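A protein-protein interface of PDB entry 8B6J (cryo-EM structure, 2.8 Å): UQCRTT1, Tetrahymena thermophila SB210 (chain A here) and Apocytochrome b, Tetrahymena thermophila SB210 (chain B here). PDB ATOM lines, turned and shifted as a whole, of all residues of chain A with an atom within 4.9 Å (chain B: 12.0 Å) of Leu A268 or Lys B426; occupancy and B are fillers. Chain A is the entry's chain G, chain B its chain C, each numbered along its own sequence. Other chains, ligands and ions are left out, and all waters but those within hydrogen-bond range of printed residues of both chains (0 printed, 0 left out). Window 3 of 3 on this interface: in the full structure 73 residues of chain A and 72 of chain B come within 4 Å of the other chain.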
ATOM      1  N   ARG A 264     -25.132  23.384 -36.793  1.00  0.00           N
ATOM      2  CA  ARG A 264     -24.435  23.843 -35.597  1.00  0.00           C
ATOM      3  C   ARG A 264     -24.829  23.013 -34.382  1.00  0.00           C
ATOM      4  O   ARG A 264     -23.988  22.705 -33.533  1.00  0.00           O
ATOM      5  CB  ARG A 264     -24.729  25.323 -35.357  1.00  0.00           C
ATOM      6  CG  ARG A 264     -23.724  26.005 -34.451  1.00  0.00           C
ATOM      7  CD  ARG A 264     -24.091  27.457 -34.203  1.00  0.00           C
ATOM      8  NE  ARG A 264     -23.043  28.166 -33.480  1.00  0.00           N
ATOM      9  CZ  ARG A 264     -23.151  29.409 -33.031  1.00  0.00           C
ATOM     10  NH1 ARG A 264     -24.261  30.110 -33.197  1.00  0.00           N
ATOM     11  NH2 ARG A 264     -22.120  29.961 -32.399  1.00  0.00           N
ATOM     12  N   PHE A 265     -26.108  22.646 -34.278  1.00  0.00           N
ATOM     13  CA  PHE A 265     -26.546  21.806 -33.168  1.00  0.00           C
ATOM     14  C   PHE A 265     -25.881  20.435 -33.218  1.00  0.00           C
ATOM     15  O   PHE A 265     -25.461  19.900 -32.183  1.00  0.00           O
ATOM     16  CB  PHE A 265     -28.066  21.662 -33.190  1.00  0.00           C
ATOM     17  CG  PHE A 265     -28.600  20.721 -32.152  1.00  0.00           C
ATOM     18  CD1 PHE A 265     -28.632  21.089 -30.818  1.00  0.00           C
ATOM     19  CD2 PHE A 265     -29.071  19.470 -32.508  1.00  0.00           C
ATOM     20  CE1 PHE A 265     -29.122  20.226 -29.859  1.00  0.00           C
ATOM     21  CE2 PHE A 265     -29.561  18.603 -31.553  1.00  0.00           C
ATOM     22  CZ  PHE A 265     -29.588  18.982 -30.227  1.00  0.00           C
ATOM     23  N   TYR A 266     -25.788  19.846 -34.411  1.00  0.00           N
ATOM     24  CA  TYR A 266     -25.110  18.561 -34.544  1.00  0.00           C
ATOM     25  C   TYR A 266     -23.639  18.680 -34.169  1.00  0.00           C
ATOM     26  O   TYR A 266     -23.086  17.794 -33.508  1.00  0.00           O
ATOM     27  CB  TYR A 266     -25.260  18.032 -35.971  1.00  0.00           C
ATOM     28  CG  TYR A 266     -26.686  17.727 -36.376  1.00  0.00           C
ATOM     29  CD1 TYR A 266     -27.625  17.311 -35.441  1.00  0.00           C
ATOM     30  CD2 TYR A 266     -27.093  17.855 -37.696  1.00  0.00           C
ATOM     31  CE1 TYR A 266     -28.924  17.031 -35.809  1.00  0.00           C
ATOM     32  CE2 TYR A 266     -28.391  17.577 -38.073  1.00  0.00           C
ATOM     33  CZ  TYR A 266     -29.302  17.165 -37.125  1.00  0.00           C
ATOM     34  OH  TYR A 266     -30.598  16.888 -37.494  1.00  0.00           O
ATOM     35  N   ALA A 267     -22.988  19.767 -34.589  1.00  0.00           N
ATOM     36  CA  ALA A 267     -21.597  19.982 -34.204  1.00  0.00           C
ATOM     37  C   ALA A 267     -21.460  20.101 -32.692  1.00  0.00           C
ATOM     38  O   ALA A 267     -20.533  19.537 -32.097  1.00  0.00           O
ATOM     39  CB  ALA A 267     -21.050  21.232 -34.891  1.00  0.00           C
ATOM     40  N   LEU A 268     -22.373  20.836 -32.053  1.00  0.00           N
ATOM     41  CA  LEU A 268     -22.350  20.959 -30.599  1.00  0.00           C
ATOM     42  C   LEU A 268     -22.472  19.595 -29.937  1.00  0.00           C
ATOM     43  O   LEU A 268     -21.699  19.258 -29.031  1.00  0.00           O
ATOM     44  CB  LEU A 268     -23.485  21.874 -30.135  1.00  0.00           C
ATOM     45  CG  LEU A 268     -23.188  23.370 -30.052  1.00  0.00           C
ATOM     46  CD1 LEU A 268     -24.479  24.161 -29.929  1.00  0.00           C
ATOM     47  CD2 LEU A 268     -22.272  23.662 -28.875  1.00  0.00           C
ATOM     48  N   GLU A 269     -23.444  18.794 -30.375  1.00  0.00           N
ATOM     49  CA  GLU A 269     -23.647  17.486 -29.761  1.00  0.00           C
ATOM     50  C   GLU A 269     -22.436  16.586 -29.966  1.00  0.00           C
ATOM     51  O   GLU A 269     -22.024  15.871 -29.047  1.00  0.00           O
ATOM     52  CB  GLU A 269     -24.906  16.830 -30.320  1.00  0.00           C
ATOM     53  CG  GLU A 269     -26.191  17.360 -29.711  1.00  0.00           C
ATOM     54  CD  GLU A 269     -27.406  16.558 -30.127  1.00  0.00           C
ATOM     55  OE1 GLU A 269     -27.409  16.022 -31.255  1.00  0.00           O
ATOM     56  OE2 GLU A 269     -28.357  16.459 -29.325  1.00  0.00           O
ATOM     57  N   ASP A 270     -21.853  16.602 -31.167  1.00  0.00           N
ATOM     58  CA  ASP A 270     -20.689  15.761 -31.424  1.00  0.00           C
ATOM     59  C   ASP A 270     -19.498  16.188 -30.577  1.00  0.00           C
ATOM     60  O   ASP A 270     -18.800  15.340 -30.009  1.00  0.00           O
ATOM     61  CB  ASP A 270     -20.336  15.791 -32.909  1.00  0.00           C
ATOM     62  CG  ASP A 270     -21.338  15.037 -33.758  1.00  0.00           C
ATOM     63  OD1 ASP A 270     -22.360  14.580 -33.204  1.00  0.00           O
ATOM     64  OD2 ASP A 270     -21.103  14.893 -34.974  1.00  0.00           O
ATOM     65  N   LEU A 271     -19.246  17.495 -30.473  1.00  0.00           N
ATOM     66  CA  LEU A 271     -18.141  17.961 -29.643  1.00  0.00           C
ATOM     67  C   LEU A 271     -18.370  17.609 -28.180  1.00  0.00           C
ATOM     68  O   LEU A 271     -17.430  17.232 -27.470  1.00  0.00           O
ATOM     69  CB  LEU A 271     -17.953  19.470 -29.807  1.00  0.00           C
ATOM     70  CG  LEU A 271     -17.441  19.947 -31.168  1.00  0.00           C
ATOM     71  CD1 LEU A 271     -17.327  21.461 -31.185  1.00  0.00           C
ATOM     72  CD2 LEU A 271     -16.105  19.305 -31.510  1.00  0.00           C
ATOM     73  N   ALA A 272     -19.613  17.727 -27.709  1.00  0.00           N
ATOM     74  CA  ALA A 272     -19.912  17.368 -26.327  1.00  0.00           C
ATOM     75  C   ALA A 272     -19.612  15.898 -26.066  1.00  0.00           C
ATOM     76  O   ALA A 272     -19.042  15.547 -25.026  1.00  0.00           O
ATOM     77  CB  ALA A 272     -21.372  17.681 -26.009  1.00  0.00           C
ATOM     78  N   VAL A 288     -18.444  27.115 -32.921  1.00  0.00           N
ATOM     79  CA  VAL A 288     -19.202  26.380 -31.914  1.00  0.00           C
ATOM     80  C   VAL A 288     -18.433  26.338 -30.601  1.00  0.00           C
ATOM     81  O   VAL A 288     -18.998  26.557 -29.525  1.00  0.00           O
ATOM     82  CB  VAL A 288     -19.529  24.963 -32.420  1.00  0.00           C
ATOM     83  CG1 VAL A 288     -20.064  24.111 -31.287  1.00  0.00           C
ATOM     84  CG2 VAL A 288     -20.535  25.029 -33.554  1.00  0.00           C
ATOM     85  N   LEU A 292     -19.646  28.059 -27.149  1.00  0.00           N
ATOM     86  CA  LEU A 292     -19.839  27.240 -25.958  1.00  0.00           C
ATOM     87  C   LEU A 292     -19.021  27.773 -24.792  1.00  0.00           C
ATOM     88  O   LEU A 292     -19.490  27.787 -23.648  1.00  0.00           O
ATOM     89  CB  LEU A 292     -19.469  25.787 -26.259  1.00  0.00           C
ATOM     90  CG  LEU A 292     -19.652  24.791 -25.112  1.00  0.00           C
ATOM     91  CD1 LEU A 292     -21.096  24.766 -24.639  1.00  0.00           C
ATOM     92  CD2 LEU A 292     -19.203  23.401 -25.536  1.00  0.00           C
ATOM     93  N   ASN B 416     -41.626  21.200 -19.428  1.00  0.00           N
ATOM     94  CA  ASN B 416     -41.387  20.486 -20.678  1.00  0.00           C
ATOM     95  C   ASN B 416     -40.831  21.431 -21.737  1.00  0.00           C
ATOM     96  O   ASN B 416     -39.837  21.124 -22.412  1.00  0.00           O
ATOM     97  CB  ASN B 416     -42.685  19.840 -21.163  1.00  0.00           C
ATOM     98  CG  ASN B 416     -42.474  18.919 -22.345  1.00  0.00           C
ATOM     99  OD1 ASN B 416     -41.394  18.359 -22.526  1.00  0.00           O
ATOM    100  ND2 ASN B 416     -43.510  18.754 -23.157  1.00  0.00           N
ATOM    101  N   ALA B 417     -41.460  22.597 -21.881  1.00  0.00           N
ATOM    102  CA  ALA B 417     -40.989  23.581 -22.850  1.00  0.00           C
ATOM    103  C   ALA B 417     -39.583  24.060 -22.507  1.00  0.00           C
ATOM    104  O   ALA B 417     -38.746  24.239 -23.398  1.00  0.00           O
ATOM    105  CB  ALA B 417     -41.957  24.761 -22.913  1.00  0.00           C
ATOM    106  N   PHE B 418     -39.310  24.284 -21.220  1.00  0.00           N
ATOM    107  CA  PHE B 418     -37.982  24.725 -20.809  1.00  0.00           C
ATOM    108  C   PHE B 418     -36.929  23.698 -21.194  1.00  0.00           C
ATOM    109  O   PHE B 418     -35.874  24.043 -21.738  1.00  0.00           O
ATOM    110  CB  PHE B 418     -37.938  24.965 -19.298  1.00  0.00           C
ATOM    111  CG  PHE B 418     -38.899  26.010 -18.804  1.00  0.00           C
ATOM    112  CD1 PHE B 418     -39.529  26.881 -19.676  1.00  0.00           C
ATOM    113  CD2 PHE B 418     -39.164  26.120 -17.450  1.00  0.00           C
ATOM    114  CE1 PHE B 418     -40.405  27.836 -19.204  1.00  0.00           C
ATOM    115  CE2 PHE B 418     -40.037  27.071 -16.975  1.00  0.00           C
ATOM    116  CZ  PHE B 418     -40.659  27.929 -17.850  1.00  0.00           C
ATOM    117  N   VAL B 419     -37.199  22.424 -20.908  1.00  0.00           N
ATOM    118  CA  VAL B 419     -36.234  21.375 -21.219  1.00  0.00           C
ATOM    119  C   VAL B 419     -36.003  21.300 -22.720  1.00  0.00           C
ATOM    120  O   VAL B 419     -34.858  21.208 -23.180  1.00  0.00           O
ATOM    121  CB  VAL B 419     -36.708  20.025 -20.651  1.00  0.00           C
ATOM    122  CG1 VAL B 419     -35.827  18.898 -21.160  1.00  0.00           C
ATOM    123  CG2 VAL B 419     -36.702  20.061 -19.133  1.00  0.00           C
ATOM    124  N   LYS B 420     -37.079  21.348 -23.510  1.00  0.00           N
ATOM    125  CA  LYS B 420     -36.918  21.268 -24.960  1.00  0.00           C
ATOM    126  C   LYS B 420     -36.101  22.443 -25.488  1.00  0.00           C
ATOM    127  O   LYS B 420     -35.178  22.264 -26.293  1.00  0.00           O
ATOM    128  CB  LYS B 420     -38.287  21.218 -25.637  1.00  0.00           C
ATOM    129  CG  LYS B 420     -39.035  19.917 -25.414  1.00  0.00           C
ATOM    130  CD  LYS B 420     -40.340  19.889 -26.185  1.00  0.00           C
ATOM    131  CE  LYS B 420     -41.052  18.560 -26.015  1.00  0.00           C
ATOM    132  NZ  LYS B 420     -42.333  18.514 -26.770  1.00  0.00           N
ATOM    133  N   SER B 421     -36.424  23.659 -25.042  1.00  0.00           N
ATOM    134  CA  SER B 421     -35.709  24.834 -25.524  1.00  0.00           C
ATOM    135  C   SER B 421     -34.240  24.787 -25.130  1.00  0.00           C
ATOM    136  O   SER B 421     -33.360  25.083 -25.949  1.00  0.00           O
ATOM    137  CB  SER B 421     -36.367  26.103 -24.986  1.00  0.00           C
ATOM    138  OG  SER B 421     -36.354  26.118 -23.571  1.00  0.00           O
ATOM    139  N   LYS B 422     -33.950  24.419 -23.880  1.00  0.00           N
ATOM    140  CA  LYS B 422     -32.560  24.361 -23.440  1.00  0.00           C
ATOM    141  C   LYS B 422     -31.791  23.289 -24.197  1.00  0.00           C
ATOM    142  O   LYS B 422     -30.626  23.492 -24.555  1.00  0.00           O
ATOM    143  CB  LYS B 422     -32.493  24.112 -21.934  1.00  0.00           C
ATOM    144  CG  LYS B 422     -31.100  24.285 -21.353  1.00  0.00           C
ATOM    145  CD  LYS B 422     -31.105  24.200 -19.837  1.00  0.00           C
ATOM    146  CE  LYS B 422     -29.718  24.453 -19.265  1.00  0.00           C
ATOM    147  NZ  LYS B 422     -29.704  24.419 -17.777  1.00  0.00           N
ATOM    148  N   PHE B 423     -32.422  22.140 -24.449  1.00  0.00           N
ATOM    149  CA  PHE B 423     -31.763  21.104 -25.235  1.00  0.00           C
ATOM    150  C   PHE B 423     -31.453  21.599 -26.640  1.00  0.00           C
ATOM    151  O   PHE B 423     -30.356  21.364 -27.161  1.00  0.00           O
ATOM    152  CB  PHE B 423     -32.640  19.854 -25.288  1.00  0.00           C
ATOM    153  CG  PHE B 423     -32.105  18.776 -26.180  1.00  0.00           C
ATOM    154  CD1 PHE B 423     -31.109  17.924 -25.739  1.00  0.00           C
ATOM    155  CD2 PHE B 423     -32.601  18.610 -27.461  1.00  0.00           C
ATOM    156  CE1 PHE B 423     -30.615  16.930 -26.558  1.00  0.00           C
ATOM    157  CE2 PHE B 423     -32.112  17.616 -28.284  1.00  0.00           C
ATOM    158  CZ  PHE B 423     -31.119  16.776 -27.832  1.00  0.00           C
ATOM    159  N   LEU B 424     -32.403  22.294 -27.270  1.00  0.00           N
ATOM    160  CA  LEU B 424     -32.156  22.813 -28.611  1.00  0.00           C
ATOM    161  C   LEU B 424     -31.019  23.827 -28.610  1.00  0.00           C
ATOM    162  O   LEU B 424     -30.146  23.791 -29.486  1.00  0.00           O
ATOM    163  CB  LEU B 424     -33.427  23.443 -29.180  1.00  0.00           C
ATOM    164  CG  LEU B 424     -34.569  22.487 -29.531  1.00  0.00           C
ATOM    165  CD1 LEU B 424     -35.720  23.251 -30.154  1.00  0.00           C
ATOM    166  CD2 LEU B 424     -34.095  21.385 -30.462  1.00  0.00           C
ATOM    167  N   LYS B 425     -31.010  24.738 -27.639  1.00  0.00           N
ATOM    168  CA  LYS B 425     -29.992  25.776 -27.564  1.00  0.00           C
ATOM    169  C   LYS B 425     -28.874  25.442 -26.587  1.00  0.00           C
ATOM    170  O   LYS B 425     -27.958  26.251 -26.415  1.00  0.00           O
ATOM    171  CB  LYS B 425     -30.634  27.111 -27.174  1.00  0.00           C
ATOM    172  CG  LYS B 425     -29.815  28.339 -27.549  1.00  0.00           C
ATOM    173  CD  LYS B 425     -29.735  28.524 -29.058  1.00  0.00           C
ATOM    174  CE  LYS B 425     -28.946  29.769 -29.425  1.00  0.00           C
ATOM    175  NZ  LYS B 425     -28.894  29.980 -30.897  1.00  0.00           N
ATOM    176  N   LYS B 426     -28.922  24.276 -25.948  1.00  0.00           N
ATOM    177  CA  LYS B 426     -27.874  23.855 -25.021  1.00  0.00           C
ATOM    178  C   LYS B 426     -27.745  24.825 -23.849  1.00  0.00           C
ATOM    179  O   LYS B 426     -27.070  24.534 -22.863  1.00  0.00           O
ATOM    180  CB  LYS B 426     -26.533  23.733 -25.749  1.00  0.00           C
ATOM    181  CG  LYS B 426     -25.448  23.059 -24.926  1.00  0.00           C
ATOM    182  CD  LYS B 426     -24.168  22.885 -25.725  1.00  0.00           C
ATOM    183  CE  LYS B 426     -23.108  22.146 -24.924  1.00  0.00           C
ATOM    184  NZ  LYS B 426     -23.519  20.755 -24.591  1.00  0.00           N
ATOM    185  OXT LYS B 426     -28.310  25.917 -23.853  1.00  0.00           O
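CE1 of Phe A265 touches O of Phe B423 (3.2 Å).
Leu B424 touches Phe A265.
Leu A268 touches Lys B426 (CD2 to CD, 3.8 Å).
CZ of Phe B423 touches OE2 of Glu A269, at 3.2 Å.
Lys B426 touches Leu A292 (CE to CD1, 3.3 Å).
Of chain B, only Lys B426 (3.8 Å) comes within 4 Å of Leu A268.
Printed residues of chain A within 4 Å of Lys B426: Leu A268 and Leu A292.
Arg A264 touches none of the printed residues of chain B.
Phe A265 touches just these residues of chain B: Phe B423 and Leu B424.
No residue of chain B comes within 4 Å of Ala A267.
Glu A269 touches just one residue of chain B: Phe B423.
Asp A270 touches none of the printed residues of chain B.
No residue of chain B comes within 4 Å of Leu A271.
Of chain B, only Lys B426 comes within 4 Å of Leu A292.
Of the printed residues of chain A, Phe B423 touches Phe A265 and Glu A269.
Printed residues of chain A within 4 Å of Leu B424: Phe A265.
Asn B416 touches none of the printed residues of chain A.
The nearest residue of chain B that does not touch Leu A268 is Lys B425 (5.4 Å).
The nearest printed residue of chain A that does not touch Lys B426 is Ala A272 (4.01 Å).
Hydrophobic or aromatic side chains of chain B within 4 Å of the printed part of chain A: Phe B423.
Of the 11 printed residues of chain A, 4 touch a printed residue of chain B.
Among the printed residues, no Asp or Glu carboxylate lies within 4 Å of a Lys or Arg side-chain nitrogen of the other chain.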
